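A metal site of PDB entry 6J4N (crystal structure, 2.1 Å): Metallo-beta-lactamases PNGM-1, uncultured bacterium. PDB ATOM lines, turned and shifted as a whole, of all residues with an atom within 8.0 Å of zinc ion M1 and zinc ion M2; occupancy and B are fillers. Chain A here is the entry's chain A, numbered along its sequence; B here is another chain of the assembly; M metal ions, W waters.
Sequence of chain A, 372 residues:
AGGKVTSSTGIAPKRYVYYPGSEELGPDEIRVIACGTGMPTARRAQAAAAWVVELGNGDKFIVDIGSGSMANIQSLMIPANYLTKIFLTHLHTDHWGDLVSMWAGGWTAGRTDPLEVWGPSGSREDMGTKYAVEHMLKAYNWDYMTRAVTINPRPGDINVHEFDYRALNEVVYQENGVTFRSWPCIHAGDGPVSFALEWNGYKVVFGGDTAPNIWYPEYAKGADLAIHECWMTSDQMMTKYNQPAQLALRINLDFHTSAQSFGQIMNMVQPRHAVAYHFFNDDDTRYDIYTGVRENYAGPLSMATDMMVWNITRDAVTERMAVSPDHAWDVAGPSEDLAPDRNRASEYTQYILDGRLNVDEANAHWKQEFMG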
ATOM      1  N   GLY A  38     -14.249   5.848 -28.139  1.00  0.00           N
ATOM      2  CA  GLY A  38     -14.202   4.753 -27.166  1.00  0.00           C
ATOM      3  C   GLY A  38     -15.548   4.334 -26.613  1.00  0.00           C
ATOM      4  O   GLY A  38     -16.505   4.262 -27.364  1.00  0.00           O
ATOM      5  N   MET A  39     -15.606   4.008 -25.320  1.00  0.00           N
ATOM      6  CA  MET A  39     -16.680   3.186 -24.697  1.00  0.00           C
ATOM      7  C   MET A  39     -17.090   3.852 -23.397  1.00  0.00           C
ATOM      8  O   MET A  39     -16.415   4.787 -22.975  1.00  0.00           O
ATOM      9  CB  MET A  39     -16.112   1.813 -24.330  1.00  0.00           C
ATOM     10  CG  MET A  39     -15.648   0.998 -25.482  1.00  0.00           C
ATOM     11  SD  MET A  39     -17.104   0.179 -26.156  1.00  0.00           S
ATOM     12  CE  MET A  39     -16.393  -1.458 -26.243  1.00  0.00           C
ATOM     13  N   PRO A  40     -18.059   3.310 -22.607  1.00  0.00           N
ATOM     14  CA  PRO A  40     -18.321   3.871 -21.282  1.00  0.00           C
ATOM     15  C   PRO A  40     -17.239   3.477 -20.269  1.00  0.00           C
ATOM     16  O   PRO A  40     -17.186   4.055 -19.203  1.00  0.00           O
ATOM     17  CB  PRO A  40     -19.667   3.287 -20.846  1.00  0.00           C
ATOM     18  CG  PRO A  40     -19.860   2.065 -21.721  1.00  0.00           C
ATOM     19  CD  PRO A  40     -18.854   2.104 -22.866  1.00  0.00           C
ATOM     20  N   ALA A  48     -14.558   8.880 -24.658  1.00  0.00           N
ATOM     21  CA  ALA A  48     -15.890   8.461 -25.144  1.00  0.00           C
ATOM     22  C   ALA A  48     -16.264   9.330 -26.345  1.00  0.00           C
ATOM     23  O   ALA A  48     -15.733  10.444 -26.510  1.00  0.00           O
ATOM     24  CB  ALA A  48     -16.910   8.567 -24.072  1.00  0.00           C
ATOM     25  N   ALA A  49     -17.200   8.829 -27.129  1.00  0.00           N
ATOM     26  CA  ALA A  49     -17.710   9.413 -28.380  1.00  0.00           C
ATOM     27  C   ALA A  49     -17.827  10.931 -28.392  1.00  0.00           C
ATOM     28  O   ALA A  49     -18.595  11.489 -27.563  1.00  0.00           O
ATOM     29  CB  ALA A  49     -19.071   8.843 -28.597  1.00  0.00           C
ATOM     30  N   ASP A  64     -22.053  14.734 -30.270  1.00  0.00           N
ATOM     31  CA  ASP A  64     -21.672  13.901 -29.104  1.00  0.00           C
ATOM     32  C   ASP A  64     -20.478  14.535 -28.365  1.00  0.00           C
ATOM     33  O   ASP A  64     -19.609  15.169 -28.986  1.00  0.00           O
ATOM     34  CB  ASP A  64     -21.448  12.420 -29.472  1.00  0.00           C
ATOM     35  CG  ASP A  64     -22.746  11.689 -29.720  1.00  0.00           C
ATOM     36  OD1 ASP A  64     -23.782  12.274 -29.396  1.00  0.00           O
ATOM     37  OD2 ASP A  64     -22.725  10.522 -30.245  1.00  0.00           O
ATOM     38  N   THR A  89     -26.550  12.301 -30.041  1.00  0.00           N
ATOM     39  CA  THR A  89     -27.231  11.145 -30.666  1.00  0.00           C
ATOM     40  C   THR A  89     -28.120  10.417 -29.661  1.00  0.00           C
ATOM     41  O   THR A  89     -29.161   9.915 -30.043  1.00  0.00           O
ATOM     42  CB  THR A  89     -26.236  10.148 -31.243  1.00  0.00           C
ATOM     43  OG1 THR A  89     -25.439   9.665 -30.161  1.00  0.00           O
ATOM     44  CG2 THR A  89     -25.449  10.766 -32.375  1.00  0.00           C
ATOM     45  N   HIS A  90     -27.677  10.298 -28.436  1.00  0.00           N
ATOM     46  CA  HIS A  90     -28.503   9.684 -27.378  1.00  0.00           C
ATOM     47  C   HIS A  90     -27.904  10.021 -26.016  1.00  0.00           C
ATOM     48  O   HIS A  90     -26.860  10.667 -25.930  1.00  0.00           O
ATOM     49  CB  HIS A  90     -28.597   8.163 -27.551  1.00  0.00           C
ATOM     50  CG  HIS A  90     -27.300   7.441 -27.492  1.00  0.00           C
ATOM     51  ND1 HIS A  90     -26.292   7.674 -28.391  1.00  0.00           N
ATOM     52  CD2 HIS A  90     -26.878   6.406 -26.725  1.00  0.00           C
ATOM     53  CE1 HIS A  90     -25.312   6.822 -28.168  1.00  0.00           C
ATOM     54  NE2 HIS A  90     -25.638   6.044 -27.171  1.00  0.00           N
ATOM     55  N   LEU A  91     -28.546   9.557 -24.959  1.00  0.00           N
ATOM     56  CA  LEU A  91     -28.306  10.088 -23.593  1.00  0.00           C
ATOM     57  C   LEU A  91     -27.523   9.148 -22.690  1.00  0.00           C
ATOM     58  O   LEU A  91     -27.539   9.313 -21.462  1.00  0.00           O
ATOM     59  CB  LEU A  91     -29.665  10.458 -23.007  1.00  0.00           C
ATOM     60  CG  LEU A  91     -30.402  11.584 -23.732  1.00  0.00           C
ATOM     61  CD1 LEU A  91     -31.816  11.689 -23.175  1.00  0.00           C
ATOM     62  CD2 LEU A  91     -29.710  12.947 -23.609  1.00  0.00           C
ATOM     63  N   HIS A  92     -26.805   8.208 -23.267  1.00  0.00           N
ATOM     64  CA  HIS A  92     -25.762   7.453 -22.542  1.00  0.00           C
ATOM     65  C   HIS A  92     -24.626   8.377 -22.111  1.00  0.00           C
ATOM     66  O   HIS A  92     -24.284   9.263 -22.872  1.00  0.00           O
ATOM     67  CB  HIS A  92     -25.213   6.340 -23.404  1.00  0.00           C
ATOM     68  CG  HIS A  92     -25.977   5.076 -23.305  1.00  0.00           C
ATOM     69  ND1 HIS A  92     -26.073   4.192 -24.367  1.00  0.00           N
ATOM     70  CD2 HIS A  92     -26.596   4.486 -22.254  1.00  0.00           C
ATOM     71  CE1 HIS A  92     -26.792   3.138 -23.970  1.00  0.00           C
ATOM     72  NE2 HIS A  92     -27.119   3.304 -22.703  1.00  0.00           N
ATOM     73  N   THR A  93     -24.091   8.192 -20.903  1.00  0.00           N
ATOM     74  CA  THR A  93     -22.917   8.941 -20.394  1.00  0.00           C
ATOM     75  C   THR A  93     -21.788   8.995 -21.417  1.00  0.00           C
ATOM     76  O   THR A  93     -21.141  10.014 -21.495  1.00  0.00           O
ATOM     77  CB  THR A  93     -22.318   8.330 -19.124  1.00  0.00           C
ATOM     78  OG1 THR A  93     -21.638   7.122 -19.475  1.00  0.00           O
ATOM     79  CG2 THR A  93     -23.397   8.031 -18.105  1.00  0.00           C
ATOM     80  N   ASP A  94     -21.524   7.950 -22.184  1.00  0.00           N
ATOM     81  CA  ASP A  94     -20.359   8.052 -23.110  1.00  0.00           C
ATOM     82  C   ASP A  94     -20.695   8.915 -24.336  1.00  0.00           C
ATOM     83  O   ASP A  94     -19.862   9.010 -25.279  1.00  0.00           O
ATOM     84  CB  ASP A  94     -19.809   6.655 -23.431  1.00  0.00           C
ATOM     85  CG  ASP A  94     -20.813   5.696 -23.997  1.00  0.00           C
ATOM     86  OD1 ASP A  94     -20.492   5.090 -25.031  1.00  0.00           O
ATOM     87  OD2 ASP A  94     -21.912   5.578 -23.399  1.00  0.00           O
ATOM     88  N   HIS A  95     -21.861   9.575 -24.361  1.00  0.00           N
ATOM     89  CA  HIS A  95     -22.225  10.448 -25.485  1.00  0.00           C
ATOM     90  C   HIS A  95     -22.517  11.884 -25.033  1.00  0.00           C
ATOM     91  O   HIS A  95     -22.526  12.767 -25.922  1.00  0.00           O
ATOM     92  CB  HIS A  95     -23.336   9.765 -26.284  1.00  0.00           C
ATOM     93  CG  HIS A  95     -22.803   8.606 -27.067  1.00  0.00           C
ATOM     94  ND1 HIS A  95     -22.512   8.688 -28.409  1.00  0.00           N
ATOM     95  CD2 HIS A  95     -22.514   7.349 -26.697  1.00  0.00           C
ATOM     96  CE1 HIS A  95     -22.025   7.525 -28.825  1.00  0.00           C
ATOM     97  NE2 HIS A  95     -22.023   6.704 -27.791  1.00  0.00           N
ATOM     98  N   HIS A 187     -31.250   0.798 -29.912  1.00  0.00           N
ATOM     99  CA  HIS A 187     -30.147   0.893 -28.941  1.00  0.00           C
ATOM    100  C   HIS A 187     -30.688   1.134 -27.530  1.00  0.00           C
ATOM    101  O   HIS A 187     -31.069   2.300 -27.217  1.00  0.00           O
ATOM    102  CB  HIS A 187     -29.203   2.017 -29.409  1.00  0.00           C
ATOM    103  CG  HIS A 187     -28.034   2.179 -28.514  1.00  0.00           C
ATOM    104  ND1 HIS A 187     -27.022   1.249 -28.445  1.00  0.00           N
ATOM    105  CD2 HIS A 187     -27.730   3.152 -27.635  1.00  0.00           C
ATOM    106  CE1 HIS A 187     -26.152   1.638 -27.557  1.00  0.00           C
ATOM    107  NE2 HIS A 187     -26.562   2.815 -27.057  1.00  0.00           N
ATOM    108  N   ALA A 188     -30.753   0.051 -26.751  1.00  0.00           N
ATOM    109  CA  ALA A 188     -31.121  -0.073 -25.310  1.00  0.00           C
ATOM    110  C   ALA A 188     -32.595   0.264 -25.004  1.00  0.00           C
ATOM    111  O   ALA A 188     -33.156  -0.330 -24.086  1.00  0.00           O
ATOM    112  CB  ALA A 188     -30.203   0.739 -24.425  1.00  0.00           C
ATOM    113  N   PRO A 192     -32.610   6.941 -29.078  1.00  0.00           N
ATOM    114  CA  PRO A 192     -31.390   7.190 -29.821  1.00  0.00           C
ATOM    115  C   PRO A 192     -31.630   7.407 -31.307  1.00  0.00           C
ATOM    116  O   PRO A 192     -32.495   6.790 -31.880  1.00  0.00           O
ATOM    117  CB  PRO A 192     -30.576   5.909 -29.598  1.00  0.00           C
ATOM    118  CG  PRO A 192     -30.987   5.465 -28.208  1.00  0.00           C
ATOM    119  CD  PRO A 192     -32.468   5.801 -28.172  1.00  0.00           C
ATOM    120  N   GLY A 208     -24.057   7.543 -34.349  1.00  0.00           N
ATOM    121  CA  GLY A 208     -24.327   7.300 -32.920  1.00  0.00           C
ATOM    122  C   GLY A 208     -24.195   5.825 -32.596  1.00  0.00           C
ATOM    123  O   GLY A 208     -23.229   5.178 -33.092  1.00  0.00           O
ATOM    124  N   ASP A 209     -25.125   5.278 -31.818  1.00  0.00           N
ATOM    125  CA  ASP A 209     -25.103   3.845 -31.460  1.00  0.00           C
ATOM    126  C   ASP A 209     -26.357   3.142 -31.968  1.00  0.00           C
ATOM    127  O   ASP A 209     -27.451   3.692 -31.789  1.00  0.00           O
ATOM    128  CB  ASP A 209     -25.074   3.620 -29.954  1.00  0.00           C
ATOM    129  CG  ASP A 209     -23.772   4.006 -29.252  1.00  0.00           C
ATOM    130  OD1 ASP A 209     -22.821   4.451 -29.929  1.00  0.00           O
ATOM    131  OD2 ASP A 209     -23.744   3.869 -28.014  1.00  0.00           O
ATOM    132  N   THR A 210     -26.181   1.920 -32.460  1.00  0.00           N
ATOM    133  CA  THR A 210     -27.319   1.085 -32.876  1.00  0.00           C
ATOM    134  C   THR A 210     -26.912  -0.356 -33.226  1.00  0.00           C
ATOM    135  O   THR A 210     -25.783  -0.579 -33.728  1.00  0.00           O
ATOM    136  CB  THR A 210     -28.020   1.774 -34.048  1.00  0.00           C
ATOM    137  OG1 THR A 210     -29.253   1.141 -34.371  1.00  0.00           O
ATOM    138  CG2 THR A 210     -27.117   1.778 -35.262  1.00  0.00           C
ATOM    139  N   GLU A 229     -21.305   2.658 -35.687  1.00  0.00           N
ATOM    140  CA  GLU A 229     -20.863   1.752 -34.621  1.00  0.00           C
ATOM    141  C   GLU A 229     -20.321   0.481 -35.287  1.00  0.00           C
ATOM    142  O   GLU A 229     -20.896   0.029 -36.277  1.00  0.00           O
ATOM    143  CB  GLU A 229     -22.016   1.499 -33.643  1.00  0.00           C
ATOM    144  CG  GLU A 229     -21.919   0.157 -32.943  1.00  0.00           C
ATOM    145  CD  GLU A 229     -23.012  -0.204 -31.974  1.00  0.00           C
ATOM    146  OE1 GLU A 229     -23.709   0.714 -31.428  1.00  0.00           O
ATOM    147  OE2 GLU A 229     -23.127  -1.403 -31.711  1.00  0.00           O
ATOM    148  N   TRP A 231     -18.567  -3.161 -33.653  1.00  0.00           N
ATOM    149  CA  TRP A 231     -18.330  -3.741 -32.311  1.00  0.00           C
ATOM    150  C   TRP A 231     -17.111  -4.662 -32.305  1.00  0.00           C
ATOM    151  O   TRP A 231     -16.794  -5.289 -33.317  1.00  0.00           O
ATOM    152  CB  TRP A 231     -19.544  -4.476 -31.771  1.00  0.00           C
ATOM    153  CG  TRP A 231     -19.645  -4.371 -30.280  1.00  0.00           C
ATOM    154  CD1 TRP A 231     -19.579  -5.383 -29.363  1.00  0.00           C
ATOM    155  CD2 TRP A 231     -19.873  -3.167 -29.533  1.00  0.00           C
ATOM    156  NE1 TRP A 231     -19.762  -4.892 -28.090  1.00  0.00           N
ATOM    157  CE2 TRP A 231     -19.946  -3.532 -28.169  1.00  0.00           C
ATOM    158  CE3 TRP A 231     -20.072  -1.827 -29.889  1.00  0.00           C
ATOM    159  CZ2 TRP A 231     -20.156  -2.597 -27.161  1.00  0.00           C
ATOM    160  CZ3 TRP A 231     -20.282  -0.893 -28.881  1.00  0.00           C
ATOM    161  CH2 TRP A 231     -20.311  -1.279 -27.543  1.00  0.00           C
ATOM    162  N   HIS A 256     -25.613  -5.092 -30.689  1.00  0.00           N
ATOM    163  CA  HIS A 256     -24.597  -4.238 -31.362  1.00  0.00           C
ATOM    164  C   HIS A 256     -24.488  -4.559 -32.838  1.00  0.00           C
ATOM    165  O   HIS A 256     -24.986  -5.623 -33.294  1.00  0.00           O
ATOM    166  CB  HIS A 256     -23.251  -4.354 -30.648  1.00  0.00           C
ATOM    167  CG  HIS A 256     -23.294  -3.787 -29.273  1.00  0.00           C
ATOM    168  ND1 HIS A 256     -23.293  -2.415 -29.051  1.00  0.00           N
ATOM    169  CD2 HIS A 256     -23.399  -4.373 -28.060  1.00  0.00           C
ATOM    170  CE1 HIS A 256     -23.391  -2.195 -27.757  1.00  0.00           C
ATOM    171  NE2 HIS A 256     -23.430  -3.383 -27.118  1.00  0.00           N
ATOM    172  N   TYR A 277     -16.264   3.020 -35.697  1.00  0.00           N
ATOM    173  CA  TYR A 277     -15.825   3.532 -34.379  1.00  0.00           C
ATOM    174  C   TYR A 277     -16.522   2.745 -33.282  1.00  0.00           C
ATOM    175  O   TYR A 277     -17.356   1.861 -33.572  1.00  0.00           O
ATOM    176  CB  TYR A 277     -16.060   5.058 -34.251  1.00  0.00           C
ATOM    177  CG  TYR A 277     -17.401   5.452 -33.666  1.00  0.00           C
ATOM    178  CD1 TYR A 277     -18.576   5.197 -34.343  1.00  0.00           C
ATOM    179  CD2 TYR A 277     -17.498   6.064 -32.428  1.00  0.00           C
ATOM    180  CE1 TYR A 277     -19.807   5.557 -33.812  1.00  0.00           C
ATOM    181  CE2 TYR A 277     -18.727   6.386 -31.863  1.00  0.00           C
ATOM    182  CZ  TYR A 277     -19.878   6.146 -32.562  1.00  0.00           C
ATOM    183  OH  TYR A 277     -21.088   6.469 -32.021  1.00  0.00           O
ATOM    184  N   HIS A 278     -16.130   3.101 -32.055  1.00  0.00           N
ATOM    185  CA  HIS A 278     -16.744   2.682 -30.765  1.00  0.00           C
ATOM    186  C   HIS A 278     -16.343   1.250 -30.418  1.00  0.00           C
ATOM    187  O   HIS A 278     -17.137   0.510 -29.871  1.00  0.00           O
ATOM    188  CB  HIS A 278     -18.267   2.830 -30.864  1.00  0.00           C
ATOM    189  CG  HIS A 278     -18.963   3.023 -29.574  1.00  0.00           C
ATOM    190  ND1 HIS A 278     -18.836   2.149 -28.497  1.00  0.00           N
ATOM    191  CD2 HIS A 278     -19.895   3.931 -29.226  1.00  0.00           C
ATOM    192  CE1 HIS A 278     -19.634   2.562 -27.519  1.00  0.00           C
ATOM    193  NE2 HIS A 278     -20.311   3.643 -27.953  1.00  0.00           N
ATOM    194  N   TRP B 142     -32.696   8.318 -18.625  1.00  0.00           N
ATOM    195  CA  TRP B 142     -32.762   7.446 -19.839  1.00  0.00           C
ATOM    196  C   TRP B 142     -31.766   6.284 -19.731  1.00  0.00           C
ATOM    197  O   TRP B 142     -32.146   5.112 -19.960  1.00  0.00           O
ATOM    198  CB  TRP B 142     -32.540   8.231 -21.131  1.00  0.00           C
ATOM    199  CG  TRP B 142     -32.702   7.359 -22.349  1.00  0.00           C
ATOM    200  CD1 TRP B 142     -33.857   7.142 -23.055  1.00  0.00           C
ATOM    201  CD2 TRP B 142     -31.690   6.571 -22.988  1.00  0.00           C
ATOM    202  NE1 TRP B 142     -33.612   6.249 -24.059  1.00  0.00           N
ATOM    203  CE2 TRP B 142     -32.302   5.892 -24.064  1.00  0.00           C
ATOM    204  CE3 TRP B 142     -30.323   6.391 -22.781  1.00  0.00           C
ATOM    205  CZ2 TRP B 142     -31.600   5.021 -24.886  1.00  0.00           C
ATOM    206  CZ3 TRP B 142     -29.626   5.536 -23.602  1.00  0.00           C
ATOM    207  CH2 TRP B 142     -30.249   4.884 -24.656  1.00  0.00           C
ATOM    208  N   ASP B 143     -30.531   6.606 -19.372  1.00  0.00           N
ATOM    209  CA  ASP B 143     -29.423   5.641 -19.192  1.00  0.00           C
ATOM    210  C   ASP B 143     -29.852   4.637 -18.112  1.00  0.00           C
ATOM    211  O   ASP B 143     -29.839   3.423 -18.374  1.00  0.00           O
ATOM    212  CB  ASP B 143     -28.138   6.428 -18.835  1.00  0.00           C
ATOM    213  CG  ASP B 143     -26.854   5.613 -18.826  1.00  0.00           C
ATOM    214  OD1 ASP B 143     -26.847   4.580 -18.210  1.00  0.00           O
ATOM    215  OD2 ASP B 143     -25.848   6.049 -19.458  1.00  0.00           O
HETATM  216 ZN    ZN M   1     -25.030   4.050 -26.203  1.00  0.00          ZN
HETATM  217 ZN    ZN M   2     -22.040   4.526 -26.814  1.00  0.00          ZN
HETATM  218  O   HOH W   1     -22.930   2.053 -25.549  1.00  0.00           O
HETATM  219  O   HOH W   2     -23.386   4.709 -25.267  1.00  0.00           O
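The nearest printed residue that does not touch zinc ion M2 is His 92 (4.7 Å).
Zinc ion M2 is bound by water W2, OD2 of Asp 209, NE2 of His 278, NE2 of His 95 and OD1 of Asp 94.
The side-chain hydroxyl (OH) of Tyr 277 is in hydrogen-bond range of the side-chain carboxylate (OD1) of Asp 209, 3.4 Å away.
A ring nitrogen (ND1) of His 278 lies within hydrogen-bond range of the backbone carbonyl oxygen of Gly 38, 3.3 Å away.
ND1 of His 278 lies within hydrogen-bond range of SD of Met 39, at 3.5 Å.
OG1 of Thr 89 sits at hydrogen-bond distance from ND1 of His 90, at 2.8 Å.
A ring nitrogen (ND1) of His 95 lies within hydrogen-bond range of the side-chain carboxylate (OD2) of Asp 64 (2.6 Å).
N of Ala 49 is in hydrogen-bond range of O of Asp 94 (3.2 Å).
Zinc ion M1 is bound by water W2 (2.0 Å), ND1 of His 92 (2.1 Å), NE2 of His 187 (2.1 Å), OD2 of Asp 209 (2.2 Å) and NE2 of His 90 (2.3 Å).
Within 4 Å of zinc ion M1: His 90, His 92, His 187 and Asp 209.
The nearest printed residue that does not touch zinc ion M1 is His 95 (4.2 Å).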
